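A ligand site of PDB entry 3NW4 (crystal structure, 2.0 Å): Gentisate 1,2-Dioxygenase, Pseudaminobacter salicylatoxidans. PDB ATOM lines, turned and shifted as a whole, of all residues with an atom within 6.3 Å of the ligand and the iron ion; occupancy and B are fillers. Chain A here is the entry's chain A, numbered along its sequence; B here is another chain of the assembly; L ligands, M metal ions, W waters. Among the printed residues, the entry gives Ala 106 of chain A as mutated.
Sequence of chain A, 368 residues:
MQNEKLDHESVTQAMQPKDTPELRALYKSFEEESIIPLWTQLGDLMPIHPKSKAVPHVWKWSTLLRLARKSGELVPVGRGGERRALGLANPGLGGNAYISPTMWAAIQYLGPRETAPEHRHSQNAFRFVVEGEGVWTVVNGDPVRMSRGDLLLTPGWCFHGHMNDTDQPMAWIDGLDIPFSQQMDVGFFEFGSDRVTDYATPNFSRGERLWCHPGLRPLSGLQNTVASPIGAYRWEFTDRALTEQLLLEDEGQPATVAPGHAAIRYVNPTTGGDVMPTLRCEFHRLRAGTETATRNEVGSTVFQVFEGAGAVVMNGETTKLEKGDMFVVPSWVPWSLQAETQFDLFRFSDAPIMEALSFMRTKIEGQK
The side-chain carboxylate (OD2) of Asp 174 lies within hydrogen-bond range of an oxygen (O3) of the ligand (2.6 Å).
NE1 of Trp 104 is in hydrogen-bond range of O3 of the ligand, 2.9 Å away.
The guanidinium group (NE) of Arg 83 is in salt-bridge range of an oxygen (O2) of the ligand.
A ring nitrogen (NE2) of His 162 lies close to an oxygen (O2) of the ligand (3.3 Å).
An oxygen (O2) of the ligand sits close to the side-chain amide oxygen (OE1) of Gln 108 (3.1 Å).
The guanidinium group (NH1) of Arg 127 is in salt-bridge range of an oxygen (O2) of the ligand (3.6 Å).
O4 of the ligand is bound to the iron ion, at 1.9 Å.
An oxygen (O1) of the ligand is bound to the iron ion (2.0 Å).
The iron ion is bound by a ring nitrogen (NE2) of His 160, 2.1 Å away.
NE2 of His 119 binds the iron ion, 2.2 Å away.
A ring nitrogen (NE2) of His 121 binds the iron ion, at 2.2 Å.
Water W2 binds the iron ion (2.4 Å).
Three residues have an atom within 4 Å of the iron ion: His 119, His 121 and His 160.
The nearest printed residue that does not touch the iron ion is Arg 127 (4.02 Å).
Merely in contact with the ligand: Ala 85 (3.3 Å), Leu 176 (3.5 Å), Ala 106 (3.6 Å), Leu 38 of chain B (3.7 Å), Met 46 of chain B (3.97 Å) and Ile 178 (3.99 Å).
Hydrophobic or aromatic side chains that line the ligand: Ala 85, Trp 104, Ala 106, His 119, His 121, His 160, His 162, Leu 176, Ile 178, Leu 38 of chain B and Met 46 of chain B.
Of the 25 residues printed, 15 come within 4 Å of the ligand.
ND1 of His 160 sits at hydrogen-bond distance from OG1 of Thr 154, at 3.3 Å.
The guanidinium group (NH2) of Arg 83 lies close to a ring nitrogen (NE2) of His 119.
The side-chain amide oxygen (OE1) of Gln 108 lies close to the side-chain carboxylate (OD2) of Asp 174.
OD1 of Asp 174 is in salt-bridge range of NH1 of Arg 127 (3.0 Å).
The backbone carbonyl oxygen (O) of Ala 106 is in hydrogen-bond range of the backbone NH (N) of Asp 174 (2.9 Å).
The backbone NH of Trp 104 is in hydrogen-bond range of the backbone carbonyl oxygen of Leu 176 (2.9 Å).
O of Trp 172 lies within hydrogen-bond range of N of Gln 108, at 2.9 Å.
O of Ala 85 sits at hydrogen-bond distance from N of Leu 38 of chain B (2.9 Å).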
ATOM      1  N   GLU A  82     -14.707  31.617 -17.642  1.00  0.00           N
ATOM      2  CA  GLU A  82     -15.576  32.191 -16.556  1.00  0.00           C
ATOM      3  C   GLU A  82     -14.902  32.682 -15.268  1.00  0.00           C
ATOM      4  O   GLU A  82     -15.184  33.807 -14.798  1.00  0.00           O
ATOM      5  CB  GLU A  82     -16.774  31.278 -16.229  1.00  0.00           C
ATOM      6  CG  GLU A  82     -17.706  31.043 -17.429  1.00  0.00           C
ATOM      7  CD  GLU A  82     -18.443  32.332 -17.893  1.00  0.00           C
ATOM      8  OE1 GLU A  82     -19.314  32.830 -17.130  1.00  0.00           O
ATOM      9  OE2 GLU A  82     -18.131  32.822 -19.017  1.00  0.00           O
ATOM     10  N   ARG A  83     -14.027  31.846 -14.676  1.00  0.00           N
ATOM     11  CA  ARG A  83     -13.421  32.105 -13.362  1.00  0.00           C
ATOM     12  C   ARG A  83     -11.978  31.631 -13.353  1.00  0.00           C
ATOM     13  O   ARG A  83     -11.668  30.599 -13.916  1.00  0.00           O
ATOM     14  CB  ARG A  83     -14.184  31.308 -12.261  1.00  0.00           C
ATOM     15  CG  ARG A  83     -15.721  31.473 -12.259  1.00  0.00           C
ATOM     16  CD  ARG A  83     -16.117  32.853 -11.786  1.00  0.00           C
ATOM     17  NE  ARG A  83     -17.556  33.080 -11.655  1.00  0.00           N
ATOM     18  CZ  ARG A  83     -18.276  33.801 -12.518  1.00  0.00           C
ATOM     19  NH1 ARG A  83     -17.676  34.319 -13.593  1.00  0.00           N
ATOM     20  NH2 ARG A  83     -19.573  34.035 -12.293  1.00  0.00           N
ATOM     21  N   ALA A  85     -10.260  29.867 -11.284  1.00  0.00           N
ATOM     22  CA  ALA A  85     -10.396  28.971 -10.144  1.00  0.00           C
ATOM     23  C   ALA A  85      -9.548  27.732 -10.394  1.00  0.00           C
ATOM     24  O   ALA A  85      -9.584  27.151 -11.483  1.00  0.00           O
ATOM     25  CB  ALA A  85     -11.908  28.588  -9.914  1.00  0.00           C
ATOM     26  N   LEU A  86      -8.792  27.328  -9.399  1.00  0.00           N
ATOM     27  CA  LEU A  86      -7.863  26.197  -9.545  1.00  0.00           C
ATOM     28  C   LEU A  86      -8.458  25.072  -8.715  1.00  0.00           C
ATOM     29  O   LEU A  86      -8.432  25.116  -7.465  1.00  0.00           O
ATOM     30  CB  LEU A  86      -6.468  26.578  -9.009  1.00  0.00           C
ATOM     31  CG  LEU A  86      -5.503  27.556  -9.718  1.00  0.00           C
ATOM     32  CD1 LEU A  86      -6.141  28.925  -9.907  1.00  0.00           C
ATOM     33  CD2 LEU A  86      -4.206  27.747  -8.910  1.00  0.00           C
ATOM     34  N   TRP A 104     -16.522  19.568  -5.584  1.00  0.00           N
ATOM     35  CA  TRP A 104     -15.440  20.402  -6.124  1.00  0.00           C
ATOM     36  C   TRP A 104     -14.999  21.433  -5.071  1.00  0.00           C
ATOM     37  O   TRP A 104     -15.816  21.940  -4.328  1.00  0.00           O
ATOM     38  CB  TRP A 104     -15.934  21.113  -7.388  1.00  0.00           C
ATOM     39  CG  TRP A 104     -15.175  22.371  -7.802  1.00  0.00           C
ATOM     40  CD1 TRP A 104     -15.272  23.612  -7.234  1.00  0.00           C
ATOM     41  CD2 TRP A 104     -14.291  22.502  -8.902  1.00  0.00           C
ATOM     42  NE1 TRP A 104     -14.468  24.508  -7.908  1.00  0.00           N
ATOM     43  CE2 TRP A 104     -13.851  23.855  -8.938  1.00  0.00           C
ATOM     44  CE3 TRP A 104     -13.839  21.617  -9.897  1.00  0.00           C
ATOM     45  CZ2 TRP A 104     -12.979  24.342  -9.920  1.00  0.00           C
ATOM     46  CZ3 TRP A 104     -12.955  22.096 -10.877  1.00  0.00           C
ATOM     47  CH2 TRP A 104     -12.542  23.454 -10.883  1.00  0.00           C
ATOM     48  N   ALA A 105     -13.679  21.673  -4.988  1.00  0.00           N
ATOM     49  CA  ALA A 105     -13.116  22.745  -4.155  1.00  0.00           C
ATOM     50  C   ALA A 105     -12.039  23.435  -4.971  1.00  0.00           C
ATOM     51  O   ALA A 105     -11.310  22.797  -5.713  1.00  0.00           O
ATOM     52  CB  ALA A 105     -12.504  22.184  -2.895  1.00  0.00           C
ATOM     53  N   ALA A 106     -11.929  24.755  -4.838  1.00  0.00           N
ATOM     54  CA  ALA A 106     -10.980  25.464  -5.642  1.00  0.00           C
ATOM     55  C   ALA A 106     -10.482  26.637  -4.890  1.00  0.00           C
ATOM     56  O   ALA A 106     -11.218  27.206  -4.089  1.00  0.00           O
ATOM     57  CB  ALA A 106     -11.645  25.960  -6.937  1.00  0.00           C
ATOM     58  N   GLN A 108      -9.803  30.406  -5.784  1.00  0.00           N
ATOM     59  CA  GLN A 108     -10.100  31.339  -6.852  1.00  0.00           C
ATOM     60  C   GLN A 108      -9.372  32.651  -6.568  1.00  0.00           C
ATOM     61  O   GLN A 108      -9.255  33.078  -5.420  1.00  0.00           O
ATOM     62  CB  GLN A 108     -11.599  31.555  -7.046  1.00  0.00           C
ATOM     63  CG  GLN A 108     -11.873  32.565  -8.190  1.00  0.00           C
ATOM     64  CD  GLN A 108     -13.316  32.690  -8.573  1.00  0.00           C
ATOM     65  OE1 GLN A 108     -14.165  31.870  -8.182  1.00  0.00           O
ATOM     66  NE2 GLN A 108     -13.619  33.680  -9.355  1.00  0.00           N
ATOM     67  N   HIS A 119     -23.220  34.524 -14.440  1.00  0.00           N
ATOM     68  CA  HIS A 119     -23.809  33.315 -15.038  1.00  0.00           C
ATOM     69  C   HIS A 119     -24.683  32.612 -13.987  1.00  0.00           C
ATOM     70  O   HIS A 119     -24.722  33.042 -12.837  1.00  0.00           O
ATOM     71  CB  HIS A 119     -22.725  32.398 -15.614  1.00  0.00           C
ATOM     72  CG  HIS A 119     -21.821  31.792 -14.587  1.00  0.00           C
ATOM     73  ND1 HIS A 119     -20.473  31.602 -14.819  1.00  0.00           N
ATOM     74  CD2 HIS A 119     -22.062  31.329 -13.333  1.00  0.00           C
ATOM     75  CE1 HIS A 119     -19.911  31.070 -13.740  1.00  0.00           C
ATOM     76  NE2 HIS A 119     -20.854  30.908 -12.820  1.00  0.00           N
ATOM     77  N   ARG A 120     -25.410  31.556 -14.377  1.00  0.00           N
ATOM     78  CA  ARG A 120     -26.082  30.708 -13.373  1.00  0.00           C
ATOM     79  C   ARG A 120     -26.023  29.270 -13.825  1.00  0.00           C
ATOM     80  O   ARG A 120     -25.855  28.984 -15.015  1.00  0.00           O
ATOM     81  CB  ARG A 120     -27.530  31.131 -13.108  1.00  0.00           C
ATOM     82  CG  ARG A 120     -28.474  30.960 -14.321  1.00  0.00           C
ATOM     83  CD  ARG A 120     -29.881  31.455 -13.957  1.00  0.00           C
ATOM     84  NE  ARG A 120     -30.798  31.492 -15.099  1.00  0.00           N
ATOM     85  CZ  ARG A 120     -32.082  31.857 -15.039  1.00  0.00           C
ATOM     86  NH1 ARG A 120     -32.822  31.900 -16.145  1.00  0.00           N
ATOM     87  NH2 ARG A 120     -32.624  32.225 -13.894  1.00  0.00           N
ATOM     88  N   HIS A 121     -26.184  28.352 -12.876  1.00  0.00           N
ATOM     89  CA  HIS A 121     -26.115  26.920 -13.167  1.00  0.00           C
ATOM     90  C   HIS A 121     -26.843  26.128 -12.108  1.00  0.00           C
ATOM     91  O   HIS A 121     -27.028  26.618 -10.987  1.00  0.00           O
ATOM     92  CB  HIS A 121     -24.649  26.492 -13.285  1.00  0.00           C
ATOM     93  CG  HIS A 121     -23.741  27.191 -12.323  1.00  0.00           C
ATOM     94  ND1 HIS A 121     -23.771  26.964 -10.963  1.00  0.00           N
ATOM     95  CD2 HIS A 121     -22.755  28.101 -12.531  1.00  0.00           C
ATOM     96  CE1 HIS A 121     -22.851  27.720 -10.367  1.00  0.00           C
ATOM     97  NE2 HIS A 121     -22.228  28.419 -11.295  1.00  0.00           N
ATOM     98  N   ALA A 125     -23.392  26.249  -4.909  1.00  0.00           N
ATOM     99  CA  ALA A 125     -22.049  26.764  -4.690  1.00  0.00           C
ATOM    100  C   ALA A 125     -21.964  27.621  -3.451  1.00  0.00           C
ATOM    101  O   ALA A 125     -22.941  28.251  -3.072  1.00  0.00           O
ATOM    102  CB  ALA A 125     -21.572  27.635  -5.939  1.00  0.00           C
ATOM    103  N   ARG A 127     -18.792  30.302  -1.250  1.00  0.00           N
ATOM    104  CA  ARG A 127     -17.456  30.905  -1.150  1.00  0.00           C
ATOM    105  C   ARG A 127     -17.017  30.989   0.321  1.00  0.00           C
ATOM    106  O   ARG A 127     -17.787  31.403   1.187  1.00  0.00           O
ATOM    107  CB  ARG A 127     -17.453  32.342  -1.720  1.00  0.00           C
ATOM    108  CG  ARG A 127     -18.415  32.599  -2.892  1.00  0.00           C
ATOM    109  CD  ARG A 127     -18.046  31.765  -4.103  1.00  0.00           C
ATOM    110  NE  ARG A 127     -19.081  31.804  -5.143  1.00  0.00           N
ATOM    111  CZ  ARG A 127     -19.200  30.882  -6.090  1.00  0.00           C
ATOM    112  NH1 ARG A 127     -18.366  29.843  -6.080  1.00  0.00           N
ATOM    113  NH2 ARG A 127     -20.171  30.976  -6.990  1.00  0.00           N
ATOM    114  N   THR A 154     -24.225  30.830  -2.960  1.00  0.00           N
ATOM    115  CA  THR A 154     -24.865  31.074  -4.237  1.00  0.00           C
ATOM    116  C   THR A 154     -25.581  29.785  -4.670  1.00  0.00           C
ATOM    117  O   THR A 154     -24.991  28.909  -5.340  1.00  0.00           O
ATOM    118  CB  THR A 154     -23.962  31.790  -5.307  1.00  0.00           C
ATOM    119  OG1 THR A 154     -24.339  31.408  -6.640  1.00  0.00           O
ATOM    120  CG2 THR A 154     -22.512  31.503  -5.073  1.00  0.00           C
ATOM    121  N   HIS A 160     -24.875  35.034 -10.636  1.00  0.00           N
ATOM    122  CA  HIS A 160     -23.787  35.542  -9.824  1.00  0.00           C
ATOM    123  C   HIS A 160     -22.626  35.960 -10.708  1.00  0.00           C
ATOM    124  O   HIS A 160     -22.332  35.315 -11.716  1.00  0.00           O
ATOM    125  CB  HIS A 160     -23.317  34.520  -8.763  1.00  0.00           C
ATOM    126  CG  HIS A 160     -22.928  33.175  -9.313  1.00  0.00           C
ATOM    127  ND1 HIS A 160     -23.865  32.285  -9.797  1.00  0.00           N
ATOM    128  CD2 HIS A 160     -21.726  32.555  -9.423  1.00  0.00           C
ATOM    129  CE1 HIS A 160     -23.256  31.167 -10.173  1.00  0.00           C
ATOM    130  NE2 HIS A 160     -21.964  31.298  -9.954  1.00  0.00           N
ATOM    131  N   HIS A 162     -18.709  38.557  -9.921  1.00  0.00           N
ATOM    132  CA  HIS A 162     -17.905  39.184  -8.853  1.00  0.00           C
ATOM    133  C   HIS A 162     -16.986  40.233  -9.434  1.00  0.00           C
ATOM    134  O   HIS A 162     -16.580  40.119 -10.605  1.00  0.00           O
ATOM    135  CB  HIS A 162     -16.982  38.215  -8.101  1.00  0.00           C
ATOM    136  CG  HIS A 162     -17.270  36.761  -8.296  1.00  0.00           C
ATOM    137  ND1 HIS A 162     -16.394  35.920  -8.938  1.00  0.00           N
ATOM    138  CD2 HIS A 162     -18.284  35.979  -7.846  1.00  0.00           C
ATOM    139  CE1 HIS A 162     -16.872  34.692  -8.925  1.00  0.00           C
ATOM    140  NE2 HIS A 162     -18.017  34.696  -8.276  1.00  0.00           N
ATOM    141  N   TRP A 172      -9.950  33.305  -2.401  1.00  0.00           N
ATOM    142  CA  TRP A 172     -10.887  32.593  -1.512  1.00  0.00           C
ATOM    143  C   TRP A 172     -11.035  31.155  -1.993  1.00  0.00           C
ATOM    144  O   TRP A 172     -10.393  30.760  -2.980  1.00  0.00           O
ATOM    145  CB  TRP A 172     -12.253  33.284  -1.493  1.00  0.00           C
ATOM    146  CG  TRP A 172     -12.996  33.304  -2.829  1.00  0.00           C
ATOM    147  CD1 TRP A 172     -13.869  32.369  -3.311  1.00  0.00           C
ATOM    148  CD2 TRP A 172     -12.893  34.312  -3.843  1.00  0.00           C
ATOM    149  NE1 TRP A 172     -14.349  32.743  -4.548  1.00  0.00           N
ATOM    150  CE2 TRP A 172     -13.767  33.954  -4.894  1.00  0.00           C
ATOM    151  CE3 TRP A 172     -12.153  35.505  -3.961  1.00  0.00           C
ATOM    152  CZ2 TRP A 172     -13.912  34.737  -6.068  1.00  0.00           C
ATOM    153  CZ3 TRP A 172     -12.298  36.288  -5.135  1.00  0.00           C
ATOM    154  CH2 TRP A 172     -13.187  35.903  -6.157  1.00  0.00           C
ATOM    155  N   ASP A 174     -13.816  28.176  -3.258  1.00  0.00           N
ATOM    156  CA  ASP A 174     -15.107  27.848  -3.755  1.00  0.00           C
ATOM    157  C   ASP A 174     -15.362  26.391  -3.380  1.00  0.00           C
ATOM    158  O   ASP A 174     -14.447  25.588  -3.465  1.00  0.00           O
ATOM    159  CB  ASP A 174     -15.137  27.869  -5.262  1.00  0.00           C
ATOM    160  CG  ASP A 174     -14.852  29.195  -5.842  1.00  0.00           C
ATOM    161  OD1 ASP A 174     -15.449  30.192  -5.374  1.00  0.00           O
ATOM    162  OD2 ASP A 174     -14.069  29.235  -6.824  1.00  0.00           O
ATOM    163  N   GLY A 175     -16.602  26.070  -3.001  1.00  0.00           N
ATOM    164  CA  GLY A 175     -17.074  24.670  -2.983  1.00  0.00           C
ATOM    165  C   GLY A 175     -18.314  24.547  -3.836  1.00  0.00           C
ATOM    166  O   GLY A 175     -19.186  25.429  -3.768  1.00  0.00           O
ATOM    167  N   LEU A 176     -18.409  23.472  -4.627  1.00  0.00           N
ATOM    168  CA  LEU A 176     -19.622  23.202  -5.442  1.00  0.00           C
ATOM    169  C   LEU A 176     -19.936  21.710  -5.464  1.00  0.00           C
ATOM    170  O   LEU A 176     -19.086  20.875  -5.125  1.00  0.00           O
ATOM    171  CB  LEU A 176     -19.492  23.692  -6.902  1.00  0.00           C
ATOM    172  CG  LEU A 176     -19.520  25.207  -7.226  1.00  0.00           C
ATOM    173  CD1 LEU A 176     -18.098  25.838  -7.149  1.00  0.00           C
ATOM    174  CD2 LEU A 176     -20.137  25.491  -8.579  1.00  0.00           C
ATOM    175  N   ILE A 178     -20.308  20.193  -8.230  1.00  0.00           N
ATOM    176  CA  ILE A 178     -19.907  19.850  -9.619  1.00  0.00           C
ATOM    177  C   ILE A 178     -19.732  18.331  -9.934  1.00  0.00           C
ATOM    178  O   ILE A 178     -20.314  17.845 -10.905  1.00  0.00           O
ATOM    179  CB  ILE A 178     -18.661  20.706 -10.078  1.00  0.00           C
ATOM    180  CG1 ILE A 178     -19.109  22.135 -10.493  1.00  0.00           C
ATOM    181  CG2 ILE A 178     -17.872  20.022 -11.231  1.00  0.00           C
ATOM    182  CD1 ILE A 178     -17.905  23.130 -10.616  1.00  0.00           C
ATOM    183  N   PHE A 189     -26.768  25.227 -17.378  1.00  0.00           N
ATOM    184  CA  PHE A 189     -25.888  26.390 -17.268  1.00  0.00           C
ATOM    185  C   PHE A 189     -26.399  27.499 -18.219  1.00  0.00           C
ATOM    186  O   PHE A 189     -26.832  27.200 -19.342  1.00  0.00           O
ATOM    187  CB  PHE A 189     -24.452  26.016 -17.638  1.00  0.00           C
ATOM    188  CG  PHE A 189     -23.481  27.166 -17.556  1.00  0.00           C
ATOM    189  CD1 PHE A 189     -23.436  28.141 -18.579  1.00  0.00           C
ATOM    190  CD2 PHE A 189     -22.607  27.291 -16.462  1.00  0.00           C
ATOM    191  CE1 PHE A 189     -22.524  29.228 -18.527  1.00  0.00           C
ATOM    192  CE2 PHE A 189     -21.689  28.378 -16.386  1.00  0.00           C
ATOM    193  CZ  PHE A 189     -21.666  29.354 -17.437  1.00  0.00           C
ATOM    194  N   LEU B  38     -10.233  25.473 -13.745  1.00  0.00           N
ATOM    195  CA  LEU B  38     -11.604  25.484 -14.288  1.00  0.00           C
ATOM    196  C   LEU B  38     -11.632  25.965 -15.742  1.00  0.00           C
ATOM    197  O   LEU B  38     -12.415  25.460 -16.571  1.00  0.00           O
ATOM    198  CB  LEU B  38     -12.538  26.379 -13.457  1.00  0.00           C
ATOM    199  CG  LEU B  38     -14.005  26.469 -13.906  1.00  0.00           C
ATOM    200  CD1 LEU B  38     -14.778  25.164 -13.573  1.00  0.00           C
ATOM    201  CD2 LEU B  38     -14.667  27.694 -13.225  1.00  0.00           C
ATOM    202  N   LEU B  42     -14.281  24.184 -18.231  1.00  0.00           N
ATOM    203  CA  LEU B  42     -15.609  24.745 -17.846  1.00  0.00           C
ATOM    204  C   LEU B  42     -16.792  24.059 -18.524  1.00  0.00           C
ATOM    205  O   LEU B  42     -17.710  23.625 -17.829  1.00  0.00           O
ATOM    206  CB  LEU B  42     -15.717  26.277 -18.010  1.00  0.00           C
ATOM    207  CG  LEU B  42     -17.002  26.788 -17.308  1.00  0.00           C
ATOM    208  CD1 LEU B  42     -16.680  27.645 -16.122  1.00  0.00           C
ATOM    209  CD2 LEU B  42     -17.971  27.499 -18.199  1.00  0.00           C
ATOM    210  N   MET B  46     -19.690  21.791 -16.737  1.00  0.00           N
ATOM    211  CA  MET B  46     -20.950  22.522 -16.517  1.00  0.00           C
ATOM    212  C   MET B  46     -21.718  22.793 -17.803  1.00  0.00           C
ATOM    213  O   MET B  46     -21.798  23.943 -18.273  1.00  0.00           O
ATOM    214  CB  MET B  46     -20.688  23.833 -15.744  1.00  0.00           C
ATOM    215  CG  MET B  46     -19.831  23.632 -14.465  1.00  0.00           C
ATOM    216  SD  MET B  46     -19.610  25.161 -13.527  1.00  0.00           S
ATOM    217  CE  MET B  46     -20.979  25.018 -12.431  1.00  0.00           C
HETATM  218  O1  LIG L   1     -19.105  31.023 -10.089  1.00  0.00           O
HETATM  219  O2  LIG L   1     -17.168  31.582  -9.027  1.00  0.00           O
HETATM  220  O3  LIG L   1     -14.621  27.318  -8.507  1.00  0.00           O
HETATM  221  O4  LIG L   1     -19.203  28.722 -11.345  1.00  0.00           O
HETATM  222  C1  LIG L   1     -16.341  26.755 -10.069  1.00  0.00           C
HETATM  223  C2  LIG L   1     -17.511  27.096 -10.767  1.00  0.00           C
HETATM  224  C3  LIG L   1     -16.254  28.961  -9.036  1.00  0.00           C
HETATM  225  C4  LIG L   1     -17.939  30.731  -9.607  1.00  0.00           C
HETATM  226  C5  LIG L   1     -15.734  27.679  -9.193  1.00  0.00           C
HETATM  227  C6  LIG L   1     -18.059  28.371 -10.642  1.00  0.00           C
HETATM  228  C7  LIG L   1     -17.403  29.342  -9.743  1.00  0.00           C
HETATM  229 FE    FE M   1     -20.614  29.902 -10.840  1.00  0.00          FE
HETATM  230  O   HOH W   1     -18.925  28.103 -13.998  1.00  0.00           O
HETATM  231  O   HOH W   2     -20.291  29.021  -8.611  1.00  0.00           O
